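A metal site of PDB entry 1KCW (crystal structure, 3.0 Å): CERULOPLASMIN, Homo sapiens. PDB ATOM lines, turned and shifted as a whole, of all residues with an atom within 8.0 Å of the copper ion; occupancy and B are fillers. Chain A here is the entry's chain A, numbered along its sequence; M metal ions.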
ATOM      1  N   GLU A 272      10.314  -4.418 -23.491  1.00  0.00           N
ATOM      2  CA  GLU A 272       9.426  -4.147 -24.607  1.00  0.00           C
ATOM      3  C   GLU A 272       7.949  -4.219 -24.336  1.00  0.00           C
ATOM      4  O   GLU A 272       7.137  -4.241 -25.253  1.00  0.00           O
ATOM      5  CB  GLU A 272       9.810  -4.973 -25.821  1.00  0.00           C
ATOM      6  CG  GLU A 272       9.653  -6.434 -25.681  1.00  0.00           C
ATOM      7  CD  GLU A 272      10.398  -7.149 -26.783  1.00  0.00           C
ATOM      8  OE1 GLU A 272      11.003  -6.470 -27.642  1.00  0.00           O
ATOM      9  OE2 GLU A 272      10.412  -8.403 -26.799  1.00  0.00           O
ATOM     10  N   PRO A 299      11.047   2.670 -22.993  1.00  0.00           N
ATOM     11  CA  PRO A 299      12.322   2.553 -22.301  1.00  0.00           C
ATOM     12  C   PRO A 299      13.314   3.725 -22.536  1.00  0.00           C
ATOM     13  O   PRO A 299      13.924   3.842 -23.587  1.00  0.00           O
ATOM     14  CB  PRO A 299      12.863   1.229 -22.848  1.00  0.00           C
ATOM     15  CG  PRO A 299      11.583   0.403 -22.899  1.00  0.00           C
ATOM     16  CD  PRO A 299      10.603   1.372 -23.529  1.00  0.00           C
ATOM     17  N   PHE A 901      17.523   0.261 -37.269  1.00  0.00           N
ATOM     18  CA  PHE A 901      17.329  -0.616 -36.114  1.00  0.00           C
ATOM     19  C   PHE A 901      16.154  -1.538 -36.431  1.00  0.00           C
ATOM     20  O   PHE A 901      15.039  -1.055 -36.540  1.00  0.00           O
ATOM     21  CB  PHE A 901      17.032   0.196 -34.848  1.00  0.00           C
ATOM     22  CG  PHE A 901      18.202   1.031 -34.369  1.00  0.00           C
ATOM     23  CD1 PHE A 901      18.609   2.161 -35.057  1.00  0.00           C
ATOM     24  CD2 PHE A 901      18.897   0.677 -33.209  1.00  0.00           C
ATOM     25  CE1 PHE A 901      19.694   2.919 -34.609  1.00  0.00           C
ATOM     26  CE2 PHE A 901      19.981   1.436 -32.762  1.00  0.00           C
ATOM     27  CZ  PHE A 901      20.371   2.551 -33.458  1.00  0.00           C
ATOM     28  N   LEU A 902      16.405  -2.834 -36.594  1.00  0.00           N
ATOM     29  CA  LEU A 902      15.321  -3.757 -36.932  1.00  0.00           C
ATOM     30  C   LEU A 902      15.643  -5.162 -36.434  1.00  0.00           C
ATOM     31  O   LEU A 902      16.755  -5.660 -36.654  1.00  0.00           O
ATOM     32  CB  LEU A 902      15.150  -3.789 -38.468  1.00  0.00           C
ATOM     33  CG  LEU A 902      13.975  -4.472 -39.183  1.00  0.00           C
ATOM     34  CD1 LEU A 902      14.500  -5.489 -40.191  1.00  0.00           C
ATOM     35  CD2 LEU A 902      13.021  -5.103 -38.211  1.00  0.00           C
ATOM     36  N   VAL A 903      14.684  -5.822 -35.788  1.00  0.00           N
ATOM     37  CA  VAL A 903      14.918  -7.182 -35.308  1.00  0.00           C
ATOM     38  C   VAL A 903      14.586  -8.123 -36.463  1.00  0.00           C
ATOM     39  O   VAL A 903      13.427  -8.445 -36.703  1.00  0.00           O
ATOM     40  CB  VAL A 903      14.009  -7.474 -34.099  1.00  0.00           C
ATOM     41  CG1 VAL A 903      14.294  -8.848 -33.520  1.00  0.00           C
ATOM     42  CG2 VAL A 903      14.209  -6.436 -33.040  1.00  0.00           C
ATOM     43  N   HIS A 940      18.360  -9.586 -33.260  1.00  0.00           N
ATOM     44  CA  HIS A 940      18.112  -8.197 -32.941  1.00  0.00           C
ATOM     45  C   HIS A 940      19.348  -7.441 -33.361  1.00  0.00           C
ATOM     46  O   HIS A 940      20.271  -7.285 -32.567  1.00  0.00           O
ATOM     47  CB  HIS A 940      17.842  -8.019 -31.459  1.00  0.00           C
ATOM     48  CG  HIS A 940      16.725  -8.874 -30.925  1.00  0.00           C
ATOM     49  ND1 HIS A 940      16.567 -10.206 -31.224  1.00  0.00           N
ATOM     50  CD2 HIS A 940      15.723  -8.562 -30.075  1.00  0.00           C
ATOM     51  CE1 HIS A 940      15.491 -10.655 -30.551  1.00  0.00           C
ATOM     52  NE2 HIS A 940      14.940  -9.701 -29.837  1.00  0.00           N
ATOM     53  N   ALA A 941      19.343  -6.872 -34.568  1.00  0.00           N
ATOM     54  CA  ALA A 941      20.539  -6.198 -35.047  1.00  0.00           C
ATOM     55  C   ALA A 941      20.457  -4.752 -35.484  1.00  0.00           C
ATOM     56  O   ALA A 941      19.386  -4.233 -35.736  1.00  0.00           O
ATOM     57  CB  ALA A 941      21.089  -7.002 -36.168  1.00  0.00           C
ATOM     58  N   ILE A 972       7.200  -5.339 -31.753  1.00  0.00           N
ATOM     59  CA  ILE A 972       8.381  -5.387 -30.907  1.00  0.00           C
ATOM     60  C   ILE A 972       9.355  -4.234 -31.168  1.00  0.00           C
ATOM     61  O   ILE A 972      10.008  -3.738 -30.249  1.00  0.00           O
ATOM     62  CB  ILE A 972       9.115  -6.693 -31.229  1.00  0.00           C
ATOM     63  CG1 ILE A 972       8.248  -7.850 -30.794  1.00  0.00           C
ATOM     64  CG2 ILE A 972      10.480  -6.746 -30.627  1.00  0.00           C
ATOM     65  CD1 ILE A 972       7.307  -7.454 -29.665  1.00  0.00           C
ATOM     66  N   ASP A 973       9.434  -3.819 -32.428  1.00  0.00           N
ATOM     67  CA  ASP A 973      10.360  -2.776 -32.818  1.00  0.00           C
ATOM     68  C   ASP A 973      10.154  -1.381 -32.222  1.00  0.00           C
ATOM     69  O   ASP A 973       9.749  -0.438 -32.900  1.00  0.00           O
ATOM     70  CB  ASP A 973      10.567  -2.809 -34.340  1.00  0.00           C
ATOM     71  CG  ASP A 973      11.283  -4.119 -34.822  1.00  0.00           C
ATOM     72  OD1 ASP A 973      12.503  -4.254 -34.571  1.00  0.00           O
ATOM     73  OD2 ASP A 973      10.661  -5.037 -35.425  1.00  0.00           O
ATOM     74  N   LEU A 974      10.351  -1.322 -30.905  1.00  0.00           N
ATOM     75  CA  LEU A 974      10.329  -0.078 -30.128  1.00  0.00           C
ATOM     76  C   LEU A 974      11.835   0.021 -29.973  1.00  0.00           C
ATOM     77  O   LEU A 974      12.471  -0.922 -29.485  1.00  0.00           O
ATOM     78  CB  LEU A 974       9.768  -0.271 -28.739  1.00  0.00           C
ATOM     79  CG  LEU A 974       8.357  -0.727 -28.486  1.00  0.00           C
ATOM     80  CD1 LEU A 974       8.228  -2.173 -28.817  1.00  0.00           C
ATOM     81  CD2 LEU A 974       8.115  -0.525 -27.009  1.00  0.00           C
ATOM     82  N   HIS A 975      12.436   1.123 -30.383  1.00  0.00           N
ATOM     83  CA  HIS A 975      13.872   1.192 -30.299  1.00  0.00           C
ATOM     84  C   HIS A 975      14.263   2.558 -29.880  1.00  0.00           C
ATOM     85  O   HIS A 975      14.098   3.525 -30.612  1.00  0.00           O
ATOM     86  CB  HIS A 975      14.463   0.856 -31.650  1.00  0.00           C
ATOM     87  CG  HIS A 975      14.159  -0.525 -32.118  1.00  0.00           C
ATOM     88  ND1 HIS A 975      14.562  -1.644 -31.411  1.00  0.00           N
ATOM     89  CD2 HIS A 975      13.650  -0.920 -33.317  1.00  0.00           C
ATOM     90  CE1 HIS A 975      14.313  -2.678 -32.187  1.00  0.00           C
ATOM     91  NE2 HIS A 975      13.758  -2.292 -33.352  1.00  0.00           N
ATOM     92  N   THR A 976      14.679   2.667 -28.641  1.00  0.00           N
ATOM     93  CA  THR A 976      15.101   3.938 -28.140  1.00  0.00           C
ATOM     94  C   THR A 976      16.587   3.931 -28.334  1.00  0.00           C
ATOM     95  O   THR A 976      17.295   3.111 -27.748  1.00  0.00           O
ATOM     96  CB  THR A 976      14.738   4.032 -26.729  1.00  0.00           C
ATOM     97  OG1 THR A 976      14.603   2.698 -26.209  1.00  0.00           O
ATOM     98  CG2 THR A 976      13.420   4.723 -26.646  1.00  0.00           C
ATOM     99  N   VAL A 977      17.026   4.733 -29.295  1.00  0.00           N
ATOM    100  CA  VAL A 977      18.423   4.801 -29.626  1.00  0.00           C
ATOM    101  C   VAL A 977      19.151   5.728 -28.698  1.00  0.00           C
ATOM    102  O   VAL A 977      18.712   6.875 -28.493  1.00  0.00           O
ATOM    103  CB  VAL A 977      18.629   5.210 -31.071  1.00  0.00           C
ATOM    104  CG1 VAL A 977      20.091   5.237 -31.386  1.00  0.00           C
ATOM    105  CG2 VAL A 977      17.983   4.220 -31.972  1.00  0.00           C
ATOM    106  N   ILE A 999      12.233   5.352 -31.728  1.00  0.00           N
ATOM    107  CA  ILE A 999      12.074   4.898 -33.091  1.00  0.00           C
ATOM    108  C   ILE A 999      11.203   3.671 -33.196  1.00  0.00           C
ATOM    109  O   ILE A 999      11.392   2.705 -32.446  1.00  0.00           O
ATOM    110  CB  ILE A 999      13.456   4.676 -33.718  1.00  0.00           C
ATOM    111  CG1 ILE A 999      13.911   5.999 -34.329  1.00  0.00           C
ATOM    112  CG2 ILE A 999      13.456   3.523 -34.687  1.00  0.00           C
ATOM    113  CD1 ILE A 999      15.041   5.905 -35.245  1.00  0.00           C
ATOM    114  N   HIS A1020      23.510   1.993 -28.478  1.00  0.00           N
ATOM    115  CA  HIS A1020      22.589   0.878 -28.308  1.00  0.00           C
ATOM    116  C   HIS A1020      21.127   1.250 -28.131  1.00  0.00           C
ATOM    117  O   HIS A1020      20.793   2.426 -27.902  1.00  0.00           O
ATOM    118  CB  HIS A1020      23.007   0.037 -27.101  1.00  0.00           C
ATOM    119  CG  HIS A1020      23.035   0.794 -25.798  1.00  0.00           C
ATOM    120  ND1 HIS A1020      21.913   1.129 -25.074  1.00  0.00           N
ATOM    121  CD2 HIS A1020      24.082   1.216 -25.050  1.00  0.00           C
ATOM    122  CE1 HIS A1020      22.320   1.721 -23.933  1.00  0.00           C
ATOM    123  NE2 HIS A1020      23.638   1.792 -23.875  1.00  0.00           N
ATOM    124  N   CYS A1021      20.267   0.245 -28.281  1.00  0.00           N
ATOM    125  CA  CYS A1021      18.839   0.431 -28.073  1.00  0.00           C
ATOM    126  C   CYS A1021      18.695   0.325 -26.577  1.00  0.00           C
ATOM    127  O   CYS A1021      19.276  -0.558 -25.986  1.00  0.00           O
ATOM    128  CB  CYS A1021      18.026  -0.683 -28.712  1.00  0.00           C
ATOM    129  SG  CYS A1021      16.302  -0.363 -28.334  1.00  0.00           S
ATOM    130  N   HIS A1022      17.920   1.191 -25.961  1.00  0.00           N
ATOM    131  CA  HIS A1022      17.793   1.169 -24.507  1.00  0.00           C
ATOM    132  C   HIS A1022      16.722   0.223 -23.964  1.00  0.00           C
ATOM    133  O   HIS A1022      16.364   0.335 -22.794  1.00  0.00           O
ATOM    134  CB  HIS A1022      17.505   2.594 -24.020  1.00  0.00           C
ATOM    135  CG  HIS A1022      18.207   2.981 -22.744  1.00  0.00           C
ATOM    136  ND1 HIS A1022      18.039   2.346 -21.537  1.00  0.00           N
ATOM    137  CD2 HIS A1022      19.056   4.009 -22.499  1.00  0.00           C
ATOM    138  CE1 HIS A1022      18.779   2.987 -20.608  1.00  0.00           C
ATOM    139  NE2 HIS A1022      19.425   4.015 -21.125  1.00  0.00           N
ATOM    140  N   VAL A1023      16.177  -0.710 -24.751  1.00  0.00           N
ATOM    141  CA  VAL A1023      15.150  -1.591 -24.186  1.00  0.00           C
ATOM    142  C   VAL A1023      15.713  -2.938 -23.845  1.00  0.00           C
ATOM    143  O   VAL A1023      16.284  -3.634 -24.700  1.00  0.00           O
ATOM    144  CB  VAL A1023      13.852  -1.711 -25.067  1.00  0.00           C
ATOM    145  CG1 VAL A1023      13.824  -0.656 -26.137  1.00  0.00           C
ATOM    146  CG2 VAL A1023      13.696  -3.100 -25.649  1.00  0.00           C
ATOM    147  N   THR A1024      15.513  -3.338 -22.591  1.00  0.00           N
ATOM    148  CA  THR A1024      16.035  -4.609 -22.067  1.00  0.00           C
ATOM    149  C   THR A1024      16.222  -5.785 -23.033  1.00  0.00           C
ATOM    150  O   THR A1024      17.352  -6.100 -23.336  1.00  0.00           O
ATOM    151  CB  THR A1024      15.275  -5.049 -20.815  1.00  0.00           C
ATOM    152  OG1 THR A1024      15.270  -3.976 -19.851  1.00  0.00           O
ATOM    153  CG2 THR A1024      15.940  -6.259 -20.201  1.00  0.00           C
ATOM    154  N   ASP A1025      15.173  -6.385 -23.569  1.00  0.00           N
ATOM    155  CA  ASP A1025      15.360  -7.532 -24.471  1.00  0.00           C
ATOM    156  C   ASP A1025      16.398  -7.214 -25.553  1.00  0.00           C
ATOM    157  O   ASP A1025      17.360  -7.975 -25.758  1.00  0.00           O
ATOM    158  CB  ASP A1025      14.015  -7.960 -25.123  1.00  0.00           C
ATOM    159  CG  ASP A1025      14.176  -9.015 -26.277  1.00  0.00           C
ATOM    160  OD1 ASP A1025      14.801 -10.084 -26.034  1.00  0.00           O
ATOM    161  OD2 ASP A1025      13.636  -8.804 -27.402  1.00  0.00           O
ATOM    162  N   HIS A1026      16.265  -6.022 -26.141  1.00  0.00           N
ATOM    163  CA  HIS A1026      17.125  -5.613 -27.241  1.00  0.00           C
ATOM    164  C   HIS A1026      18.595  -5.506 -26.905  1.00  0.00           C
ATOM    165  O   HIS A1026      19.425  -5.994 -27.666  1.00  0.00           O
ATOM    166  CB  HIS A1026      16.573  -4.367 -27.891  1.00  0.00           C
ATOM    167  CG  HIS A1026      15.194  -4.567 -28.459  1.00  0.00           C
ATOM    168  ND1 HIS A1026      14.523  -3.541 -29.055  1.00  0.00           N
ATOM    169  CD2 HIS A1026      14.360  -5.613 -28.291  1.00  0.00           C
ATOM    170  CE1 HIS A1026      13.296  -3.965 -29.232  1.00  0.00           C
ATOM    171  NE2 HIS A1026      13.150  -5.212 -28.786  1.00  0.00           N
ATOM    172  N   ILE A1027      18.926  -4.965 -25.742  1.00  0.00           N
ATOM    173  CA  ILE A1027      20.324  -4.878 -25.343  1.00  0.00           C
ATOM    174  C   ILE A1027      20.919  -6.286 -25.224  1.00  0.00           C
ATOM    175  O   ILE A1027      21.834  -6.640 -25.955  1.00  0.00           O
ATOM    176  CB  ILE A1027      20.475  -4.190 -24.016  1.00  0.00           C
ATOM    177  CG1 ILE A1027      20.123  -2.724 -24.161  1.00  0.00           C
ATOM    178  CG2 ILE A1027      21.891  -4.284 -23.564  1.00  0.00           C
ATOM    179  CD1 ILE A1027      20.290  -1.931 -22.846  1.00  0.00           C
ATOM    180  N   MET A1031      21.551  -5.599 -29.899  1.00  0.00           N
ATOM    181  CA  MET A1031      21.277  -4.393 -30.634  1.00  0.00           C
ATOM    182  C   MET A1031      22.204  -3.288 -30.163  1.00  0.00           C
ATOM    183  O   MET A1031      21.752  -2.286 -29.600  1.00  0.00           O
ATOM    184  CB  MET A1031      19.803  -4.041 -30.424  1.00  0.00           C
ATOM    185  CG  MET A1031      19.246  -2.870 -31.246  1.00  0.00           C
ATOM    186  SD  MET A1031      17.519  -3.174 -31.596  1.00  0.00           S
ATOM    187  CE  MET A1031      17.783  -4.444 -32.777  1.00  0.00           C
HETATM  188 CU    CU M   1      15.491  -1.788 -29.542  1.00  0.00          CU
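Leu 974 touches the copper ion (O to CU, 3.1 Å).
Val 1023 touches the copper ion (CG1 to CU, 3.96 Å).
SD of Met 1031 touches the copper ion, 3.2 Å away.
Six residues have an atom within 4 Å of the copper ion: Leu 974, His 975, Cys 1021, Val 1023, His 1026 and Met 1031.
The nearest printed residue that does not touch the copper ion is Thr 976 (4.6 Å).
N of His 975 lies within hydrogen-bond range of O of Ile 999 (2.8 Å).
The backbone carbonyl oxygen of His 940 sits at hydrogen-bond distance from the backbone NH of Met 1031 (3.4 Å).
NE2 of His 1026 lies within hydrogen-bond range of OE1 of Glu 272, 2.7 Å away.
The side-chain sulfur (SD) of Met 1031 lies close to a ring nitrogen (ND1) of His 975 (3.3 Å).
SG of Cys 1021 lies close to N of Thr 976, at 3.5 Å.
The side-chain sulfur (SG) of Cys 1021 lies close to the backbone NH (N) of Val 1023, at 3.6 Å.
NE2 of His 975 is in hydrogen-bond range of OD1 of Asp 973 (2.6 Å).
O of His 1026 lies within hydrogen-bond range of N of Met 1031, 3.1 Å away.
The copper ion is bound by the side-chain sulfur of Cys 1021, a ring nitrogen (ND1) of His 1026 and a ring nitrogen (ND1) of His 975.
The copper ion has three donor atoms within binding distance.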
